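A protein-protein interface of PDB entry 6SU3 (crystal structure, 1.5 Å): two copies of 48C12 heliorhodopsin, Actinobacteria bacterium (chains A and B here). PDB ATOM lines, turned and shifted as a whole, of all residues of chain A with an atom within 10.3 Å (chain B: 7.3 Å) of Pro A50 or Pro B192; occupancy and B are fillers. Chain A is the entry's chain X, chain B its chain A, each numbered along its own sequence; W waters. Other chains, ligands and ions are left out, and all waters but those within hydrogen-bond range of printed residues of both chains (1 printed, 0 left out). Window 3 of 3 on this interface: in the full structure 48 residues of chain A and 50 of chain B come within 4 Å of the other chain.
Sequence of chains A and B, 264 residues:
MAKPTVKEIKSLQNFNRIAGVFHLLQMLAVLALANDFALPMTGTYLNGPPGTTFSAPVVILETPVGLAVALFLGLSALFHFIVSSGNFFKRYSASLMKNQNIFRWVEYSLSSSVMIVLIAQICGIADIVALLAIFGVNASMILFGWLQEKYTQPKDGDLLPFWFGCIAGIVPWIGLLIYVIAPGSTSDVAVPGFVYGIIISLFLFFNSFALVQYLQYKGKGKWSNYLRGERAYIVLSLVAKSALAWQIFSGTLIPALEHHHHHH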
ATOM      1  N   TYR A  45      10.663  14.972  13.996  1.00  0.00           N
ATOM      2  CA  TYR A  45       9.420  15.581  13.475  1.00  0.00           C
ATOM      3  C   TYR A  45       9.680  17.026  13.058  1.00  0.00           C
ATOM      4  O   TYR A  45      10.490  17.732  13.700  1.00  0.00           O
ATOM      5  CB  TYR A  45       8.309  15.469  14.508  1.00  0.00           C
ATOM      6  CG  TYR A  45       8.104  14.067  15.008  1.00  0.00           C
ATOM      7  CD1 TYR A  45       7.871  13.015  14.129  1.00  0.00           C
ATOM      8  CD2 TYR A  45       8.163  13.784  16.354  1.00  0.00           C
ATOM      9  CE1 TYR A  45       7.680  11.722  14.589  1.00  0.00           C
ATOM     10  CE2 TYR A  45       7.972  12.501  16.831  1.00  0.00           C
ATOM     11  CZ  TYR A  45       7.721  11.468  15.948  1.00  0.00           C
ATOM     12  OH  TYR A  45       7.542  10.203  16.422  1.00  0.00           O
ATOM     13  N   LEU A  46       8.966  17.464  12.026  1.00  0.00           N
ATOM     14  CA  LEU A  46       8.963  18.884  11.612  1.00  0.00           C
ATOM     15  C   LEU A  46       8.493  19.736  12.802  1.00  0.00           C
ATOM     16  O   LEU A  46       7.604  19.294  13.578  1.00  0.00           O
ATOM     17  CB  LEU A  46       8.075  19.047  10.376  1.00  0.00           C
ATOM     18  CG  LEU A  46       8.760  18.729   9.051  1.00  0.00           C
ATOM     19  CD1 LEU A  46       7.731  18.546   7.948  1.00  0.00           C
ATOM     20  CD2 LEU A  46       9.757  19.825   8.692  1.00  0.00           C
ATOM     21  N   ASN A  47       9.126  20.890  12.969  1.00  0.00           N
ATOM     22  CA  ASN A  47       8.834  21.872  14.043  1.00  0.00           C
ATOM     23  C   ASN A  47       8.208  23.109  13.400  1.00  0.00           C
ATOM     24  O   ASN A  47       8.543  24.215  13.824  1.00  0.00           O
ATOM     25  CB  ASN A  47      10.116  22.219  14.802  1.00  0.00           C
ATOM     26  CG  ASN A  47       9.854  22.924  16.113  1.00  0.00           C
ATOM     27  OD1 ASN A  47      10.768  23.504  16.700  1.00  0.00           O
ATOM     28  ND2 ASN A  47       8.616  22.867  16.580  1.00  0.00           N
ATOM     29  N   GLY A  48       7.357  22.905  12.395  1.00  0.00           N
ATOM     30  CA  GLY A  48       6.945  23.919  11.409  1.00  0.00           C
ATOM     31  C   GLY A  48       6.453  23.254  10.130  1.00  0.00           C
ATOM     32  O   GLY A  48       6.481  22.023  10.013  1.00  0.00           O
ATOM     33  N   PRO A  49       5.993  24.049   9.137  1.00  0.00           N
ATOM     34  CA  PRO A  49       5.618  23.515   7.831  1.00  0.00           C
ATOM     35  C   PRO A  49       6.766  22.752   7.181  1.00  0.00           C
ATOM     36  O   PRO A  49       7.935  22.937   7.519  1.00  0.00           O
ATOM     37  CB  PRO A  49       5.268  24.767   7.002  1.00  0.00           C
ATOM     38  CG  PRO A  49       4.917  25.818   8.030  1.00  0.00           C
ATOM     39  CD  PRO A  49       5.791  25.503   9.229  1.00  0.00           C
ATOM     40  N   PRO A  50       6.458  21.884   6.197  1.00  0.00           N
ATOM     41  CA  PRO A  50       7.485  21.277   5.358  1.00  0.00           C
ATOM     42  C   PRO A  50       8.426  22.356   4.807  1.00  0.00           C
ATOM     43  O   PRO A  50       7.931  23.420   4.430  1.00  0.00           O
ATOM     44  CB  PRO A  50       6.713  20.616   4.206  1.00  0.00           C
ATOM     45  CG  PRO A  50       5.281  20.536   4.659  1.00  0.00           C
ATOM     46  CD  PRO A  50       5.097  21.496   5.808  1.00  0.00           C
ATOM     47  N   GLY A  51       9.730  22.068   4.783  1.00  0.00           N
ATOM     48  CA  GLY A  51      10.758  22.963   4.213  1.00  0.00           C
ATOM     49  C   GLY A  51      11.264  23.973   5.235  1.00  0.00           C
ATOM     50  O   GLY A  51      12.019  24.874   4.843  1.00  0.00           O
ATOM     51  N   THR A  52      10.870  23.842   6.506  1.00  0.00           N
ATOM     52  CA  THR A  52      11.373  24.705   7.610  1.00  0.00           C
ATOM     53  C   THR A  52      12.381  23.896   8.429  1.00  0.00           C
ATOM     54  O   THR A  52      13.369  23.446   7.833  1.00  0.00           O
ATOM     55  CB  THR A  52      10.235  25.344   8.419  1.00  0.00           C
ATOM     56  OG1 THR A  52       9.484  24.351   9.118  1.00  0.00           O
ATOM     57  CG2 THR A  52       9.313  26.170   7.550  1.00  0.00           C
ATOM     58  N   THR A  53      12.151  23.722   9.733  1.00  0.00           N
ATOM     59  CA  THR A  53      13.148  23.141  10.671  1.00  0.00           C
ATOM     60  C   THR A  53      12.528  21.956  11.410  1.00  0.00           C
ATOM     61  O   THR A  53      11.281  21.816  11.381  1.00  0.00           O
ATOM     62  CB  THR A  53      13.684  24.184  11.664  1.00  0.00           C
ATOM     63  OG1 THR A  53      12.624  24.512  12.560  1.00  0.00           O
ATOM     64  CG2 THR A  53      14.208  25.430  10.987  1.00  0.00           C
ATOM     65  N   PHE A  54      13.384  21.134  12.022  1.00  0.00           N
ATOM     66  CA  PHE A  54      13.014  19.874  12.714  1.00  0.00           C
ATOM     67  C   PHE A  54      13.289  20.023  14.205  1.00  0.00           C
ATOM     68  O   PHE A  54      14.260  20.695  14.601  1.00  0.00           O
ATOM     69  CB  PHE A  54      13.767  18.679  12.119  1.00  0.00           C
ATOM     70  CG  PHE A  54      13.396  18.368  10.690  1.00  0.00           C
ATOM     71  CD1 PHE A  54      12.468  17.383  10.391  1.00  0.00           C
ATOM     72  CD2 PHE A  54      13.950  19.085   9.642  1.00  0.00           C
ATOM     73  CE1 PHE A  54      12.118  17.112   9.077  1.00  0.00           C
ATOM     74  CE2 PHE A  54      13.607  18.803   8.328  1.00  0.00           C
ATOM     75  CZ  PHE A  54      12.692  17.813   8.048  1.00  0.00           C
ATOM     76  N   PHE B  37      11.649  25.158  -4.189  1.00  0.00           N
ATOM     77  CA  PHE B  37      11.374  24.442  -2.916  1.00  0.00           C
ATOM     78  C   PHE B  37      12.083  23.078  -2.928  1.00  0.00           C
ATOM     79  O   PHE B  37      11.991  22.323  -3.924  1.00  0.00           O
ATOM     80  CB  PHE B  37       9.867  24.299  -2.700  1.00  0.00           C
ATOM     81  CG  PHE B  37       9.458  23.672  -1.393  1.00  0.00           C
ATOM     82  CD1 PHE B  37       9.473  24.405  -0.219  1.00  0.00           C
ATOM     83  CD2 PHE B  37       9.012  22.358  -1.341  1.00  0.00           C
ATOM     84  CE1 PHE B  37       9.081  23.828   0.978  1.00  0.00           C
ATOM     85  CE2 PHE B  37       8.624  21.783  -0.140  1.00  0.00           C
ATOM     86  CZ  PHE B  37       8.657  22.521   1.016  1.00  0.00           C
ATOM     87  N   ALA B  38      12.756  22.744  -1.825  1.00  0.00           N
ATOM     88  CA  ALA B  38      13.517  21.486  -1.681  1.00  0.00           C
ATOM     89  C   ALA B  38      13.225  20.864  -0.317  1.00  0.00           C
ATOM     90  O   ALA B  38      12.934  21.598   0.634  1.00  0.00           O
ATOM     91  CB  ALA B  38      14.991  21.735  -1.877  1.00  0.00           C
ATOM     92  N   LEU B  39      13.284  19.538  -0.246  1.00  0.00           N
ATOM     93  CA  LEU B  39      13.111  18.777   1.016  1.00  0.00           C
ATOM     94  C   LEU B  39      14.340  17.914   1.263  1.00  0.00           C
ATOM     95  O   LEU B  39      14.890  17.291   0.351  1.00  0.00           O
ATOM     96  CB  LEU B  39      11.830  17.947   0.954  1.00  0.00           C
ATOM     97  CG  LEU B  39      10.535  18.761   0.907  1.00  0.00           C
ATOM     98  CD1 LEU B  39       9.355  17.865   0.580  1.00  0.00           C
ATOM     99  CD2 LEU B  39      10.308  19.506   2.211  1.00  0.00           C
ATOM    100  N   PRO B  40      14.822  17.900   2.522  1.00  0.00           N
ATOM    101  CA  PRO B  40      16.101  17.286   2.850  1.00  0.00           C
ATOM    102  C   PRO B  40      16.030  15.757   2.953  1.00  0.00           C
ATOM    103  O   PRO B  40      15.019  15.204   3.364  1.00  0.00           O
ATOM    104  CB  PRO B  40      16.444  17.921   4.203  1.00  0.00           C
ATOM    105  CG  PRO B  40      15.099  18.192   4.831  1.00  0.00           C
ATOM    106  CD  PRO B  40      14.200  18.564   3.674  1.00  0.00           C
ATOM    107  N   GLN B 121       8.404  12.867   2.436  1.00  0.00           N
ATOM    108  CA  GLN B 121       9.217  14.086   2.710  1.00  0.00           C
ATOM    109  C   GLN B 121       8.291  15.240   3.138  1.00  0.00           C
ATOM    110  O   GLN B 121       8.670  16.017   4.044  1.00  0.00           O
ATOM    111  CB  GLN B 121      10.072  14.428   1.496  1.00  0.00           C
ATOM    112  CG  GLN B 121      11.179  13.416   1.235  1.00  0.00           C
ATOM    113  CD  GLN B 121      12.211  13.951   0.276  1.00  0.00           C
ATOM    114  OE1 GLN B 121      12.091  13.795  -0.939  1.00  0.00           O
ATOM    115  NE2 GLN B 121      13.215  14.620   0.821  1.00  0.00           N
ATOM    116  N   ILE B 122       7.126  15.373   2.506  1.00  0.00           N
ATOM    117  CA  ILE B 122       6.110  16.413   2.861  1.00  0.00           C
ATOM    118  C   ILE B 122       5.662  16.212   4.319  1.00  0.00           C
ATOM    119  O   ILE B 122       5.353  17.212   5.010  1.00  0.00           O
ATOM    120  CB  ILE B 122       4.935  16.373   1.862  1.00  0.00           C
ATOM    121  CG1 ILE B 122       5.371  16.821   0.465  1.00  0.00           C
ATOM    122  CG2 ILE B 122       3.767  17.191   2.366  1.00  0.00           C
ATOM    123  CD1 ILE B 122       5.688  18.284   0.376  1.00  0.00           C
ATOM    124  N   CYS B 123       5.639  14.970   4.792  1.00  0.00           N
ATOM    125  CA  CYS B 123       5.252  14.621   6.180  1.00  0.00           C
ATOM    126  C   CYS B 123       6.428  14.822   7.147  1.00  0.00           C
ATOM    127  O   CYS B 123       6.226  14.644   8.354  1.00  0.00           O
ATOM    128  CB  CYS B 123       4.752  13.187   6.250  1.00  0.00           C
ATOM    129  SG  CYS B 123       3.126  12.959   5.479  1.00  0.00           S
ATOM    130  N   GLY B 124       7.619  15.138   6.631  1.00  0.00           N
ATOM    131  CA  GLY B 124       8.823  15.402   7.440  1.00  0.00           C
ATOM    132  C   GLY B 124       9.708  14.178   7.619  1.00  0.00           C
ATOM    133  O   GLY B 124      10.714  14.287   8.333  1.00  0.00           O
ATOM    134  N   VAL B 189       2.617  18.424  17.371  1.00  0.00           N
ATOM    135  CA  VAL B 189       3.128  18.774  16.017  1.00  0.00           C
ATOM    136  C   VAL B 189       1.967  19.359  15.212  1.00  0.00           C
ATOM    137  O   VAL B 189       0.954  18.659  15.048  1.00  0.00           O
ATOM    138  CB  VAL B 189       3.746  17.540  15.335  1.00  0.00           C
ATOM    139  CG1 VAL B 189       4.186  17.832  13.909  1.00  0.00           C
ATOM    140  CG2 VAL B 189       4.898  16.981  16.153  1.00  0.00           C
ATOM    141  N   ALA B 190       2.117  20.601  14.752  1.00  0.00           N
ATOM    142  CA  ALA B 190       1.131  21.329  13.921  1.00  0.00           C
ATOM    143  C   ALA B 190       1.366  21.001  12.441  1.00  0.00           C
ATOM    144  O   ALA B 190       2.151  21.719  11.796  1.00  0.00           O
ATOM    145  CB  ALA B 190       1.250  22.807  14.190  1.00  0.00           C
ATOM    146  N   VAL B 191       0.712  19.950  11.934  1.00  0.00           N
ATOM    147  CA  VAL B 191       0.793  19.513  10.508  1.00  0.00           C
ATOM    148  C   VAL B 191      -0.185  20.344   9.684  1.00  0.00           C
ATOM    149  O   VAL B 191      -1.374  20.395   9.998  1.00  0.00           O
ATOM    150  CB  VAL B 191       0.501  18.013  10.348  1.00  0.00           C
ATOM    151  CG1 VAL B 191       0.548  17.595   8.884  1.00  0.00           C
ATOM    152  CG2 VAL B 191       1.439  17.161  11.187  1.00  0.00           C
ATOM    153  N   PRO B 192       0.300  21.027   8.623  1.00  0.00           N
ATOM    154  CA  PRO B 192      -0.560  21.843   7.775  1.00  0.00           C
ATOM    155  C   PRO B 192      -1.731  21.023   7.217  1.00  0.00           C
ATOM    156  O   PRO B 192      -1.564  19.826   6.927  1.00  0.00           O
ATOM    157  CB  PRO B 192       0.366  22.319   6.647  1.00  0.00           C
ATOM    158  CG  PRO B 192       1.752  22.236   7.234  1.00  0.00           C
ATOM    159  CD  PRO B 192       1.709  21.075   8.204  1.00  0.00           C
ATOM    160  N   GLY B 193      -2.885  21.677   7.064  1.00  0.00           N
ATOM    161  CA  GLY B 193      -4.052  21.098   6.373  1.00  0.00           C
ATOM    162  C   GLY B 193      -3.670  20.443   5.057  1.00  0.00           C
ATOM    163  O   GLY B 193      -4.175  19.339   4.783  1.00  0.00           O
ATOM    164  N   PHE B 194      -2.851  21.099   4.232  1.00  0.00           N
ATOM    165  CA  PHE B 194      -2.610  20.638   2.844  1.00  0.00           C
ATOM    166  C   PHE B 194      -1.873  19.298   2.895  1.00  0.00           C
ATOM    167  O   PHE B 194      -2.031  18.489   1.982  1.00  0.00           O
ATOM    168  CB  PHE B 194      -1.877  21.688   2.010  1.00  0.00           C
ATOM    169  CG  PHE B 194      -0.379  21.697   2.158  1.00  0.00           C
ATOM    170  CD1 PHE B 194       0.414  20.868   1.378  1.00  0.00           C
ATOM    171  CD2 PHE B 194       0.242  22.554   3.050  1.00  0.00           C
ATOM    172  CE1 PHE B 194       1.795  20.879   1.510  1.00  0.00           C
ATOM    173  CE2 PHE B 194       1.621  22.563   3.176  1.00  0.00           C
ATOM    174  CZ  PHE B 194       2.393  21.722   2.413  1.00  0.00           C
ATOM    175  N   VAL B 195      -1.103  19.058   3.955  1.00  0.00           N
ATOM    176  CA  VAL B 195      -0.358  17.780   4.134  1.00  0.00           C
ATOM    177  C   VAL B 195      -1.357  16.651   4.404  1.00  0.00           C
ATOM    178  O   VAL B 195      -1.256  15.596   3.778  1.00  0.00           O
ATOM    179  CB  VAL B 195       0.687  17.911   5.252  1.00  0.00           C
ATOM    180  CG1 VAL B 195       1.285  16.556   5.595  1.00  0.00           C
ATOM    181  CG2 VAL B 195       1.761  18.918   4.849  1.00  0.00           C
ATOM    182  N   TYR B 196      -2.327  16.892   5.279  1.00  0.00           N
ATOM    183  CA  TYR B 196      -3.436  15.946   5.521  1.00  0.00           C
ATOM    184  C   TYR B 196      -4.180  15.689   4.206  1.00  0.00           C
ATOM    185  O   TYR B 196      -4.470  14.522   3.911  1.00  0.00           O
ATOM    186  CB  TYR B 196      -4.344  16.474   6.623  1.00  0.00           C
ATOM    187  CG  TYR B 196      -3.751  16.348   8.004  1.00  0.00           C
ATOM    188  CD1 TYR B 196      -3.524  15.103   8.564  1.00  0.00           C
ATOM    189  CD2 TYR B 196      -3.433  17.465   8.758  1.00  0.00           C
ATOM    190  CE1 TYR B 196      -3.006  14.968   9.841  1.00  0.00           C
ATOM    191  CE2 TYR B 196      -2.910  17.349  10.037  1.00  0.00           C
ATOM    192  CZ  TYR B 196      -2.693  16.096  10.578  1.00  0.00           C
ATOM    193  OH  TYR B 196      -2.175  15.967  11.830  1.00  0.00           O
ATOM    194  N   GLY B 197      -4.457  16.732   3.425  1.00  0.00           N
ATOM    195  CA  GLY B 197      -5.140  16.586   2.126  1.00  0.00           C
ATOM    196  C   GLY B 197      -4.392  15.607   1.248  1.00  0.00           C
ATOM    197  O   GLY B 197      -5.027  14.716   0.635  1.00  0.00           O
ATOM    198  N   ILE B 198      -3.074  15.773   1.180  1.00  0.00           N
ATOM    199  CA  ILE B 198      -2.203  14.934   0.318  1.00  0.00           C
ATOM    200  C   ILE B 198      -2.275  13.486   0.804  1.00  0.00           C
ATOM    201  O   ILE B 198      -2.525  12.592  -0.011  1.00  0.00           O
ATOM    202  CB  ILE B 198      -0.772  15.483   0.273  1.00  0.00           C
ATOM    203  CG1 ILE B 198      -0.698  16.712  -0.641  1.00  0.00           C
ATOM    204  CG2 ILE B 198       0.207  14.397  -0.160  1.00  0.00           C
ATOM    205  CD1 ILE B 198       0.589  17.496  -0.519  1.00  0.00           C
ATOM    206  N   GLY B 251       0.623  23.817  -2.171  1.00  0.00           N
ATOM    207  CA  GLY B 251       1.147  23.796  -0.794  1.00  0.00           C
ATOM    208  C   GLY B 251       2.528  24.420  -0.678  1.00  0.00           C
ATOM    209  O   GLY B 251       2.811  25.012   0.393  1.00  0.00           O
ATOM    210  N   THR B 252       3.390  24.265  -1.690  1.00  0.00           N
ATOM    211  CA  THR B 252       4.853  24.449  -1.505  1.00  0.00           C
ATOM    212  C   THR B 252       5.539  25.174  -2.668  1.00  0.00           C
ATOM    213  O   THR B 252       6.650  25.662  -2.430  1.00  0.00           O
ATOM    214  CB  THR B 252       5.571  23.124  -1.215  1.00  0.00           C
ATOM    215  OG1 THR B 252       5.554  22.275  -2.366  1.00  0.00           O
ATOM    216  CG2 THR B 252       4.974  22.396  -0.033  1.00  0.00           C
HETATM  217  O   HOH W   1       7.203  15.476  10.910  1.00  0.00           O
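Leu A46 touches Val B189.
Pro A50 touches Phe B37.
CG of Pro A50 touches O of Ile B122, 3.3 Å away.
CD of Pro A50 touches CG of Pro B192 (3.7 Å).
CG of Pro A50 touches CZ of Phe B194, at 3.8 Å.
CG2 of Val B195 touches CG of Pro A50, at 3.9 Å.
CA of Gly A51 touches CE1 of Phe B37, at 3.7 Å.
Leu B39 touches Gly A51.
CE2 of Phe A54 touches CG of Pro B40, 3.9 Å away.
CE1 of Phe A54 touches O of Gly B124 (3.2 Å).
Printed residues of chain B within 4 Å of Leu A46: Gly B124 and Val B189.
Pro A50 touches just these residues of chain B: Phe B37 (3.6 Å), Ile B122 (3.3 Å), Pro B192 (3.7 Å), Phe B194 (3.8 Å) and Val B195 (3.9 Å).
Of the printed residues of chain B, Phe A54 touches Pro B40 and Gly B124.
Printed residues of chain A within 4 Å of Leu B39: Gly A51.
Printed residues of chain A within 4 Å of Ile B122: Pro A50.
Of the printed residues of chain A, Val B189 touches Leu A46.
Of chain A, only Pro A50 comes within 4 Å of Pro B192.
No residue of chain A comes within 4 Å of Gly B193.
Phe B194 touches one residue of chain A.
The nearest residue of chain B that does not touch Pro A50 is Leu B39 (4.3 Å).
The nearest printed residue of chain A that does not touch Leu B39 is Pro A50 (4.3 Å).
The backbone carbonyl oxygen (O) of Leu B39 is in hydrogen-bond range of the side-chain amide nitrogen (NE2) of Gln B121.
The side-chain amide nitrogen (NE2) of Gln B121 is in hydrogen-bond range of the backbone carbonyl oxygen (O) of Pro B40, 3.2 Å away.
No position is printed for both chains.
Of the 11 pairs that touch across the chains among the printed residues, none has its exchanged pair printed and touching as well.
Water W1 bridges the backbone carbonyl oxygen of Cys B123 and the backbone NH of Leu A46.
Hydrophobic or aromatic side chains of chain B that line the printed part of chain A: Phe B37, Leu B39, Pro B40, Val B189, Pro B192, Phe B194 and Val B195.
Along chain B the printed residues that touch a printed residue of chain A span positions 37 to 195.
Of the 10 printed residues of chain A, 4 touch a printed residue of chain B.
Hydrophobic or aromatic side chains of chain A within 4 Å of the printed part of chain B: Leu A46, Pro A50 and Phe A54.
Among the printed residues, 11 pairs touch across the chains.
Among the printed residues, no Asp or Glu carboxylate lies within 4 Å of a Lys or Arg side-chain nitrogen of the other chain.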
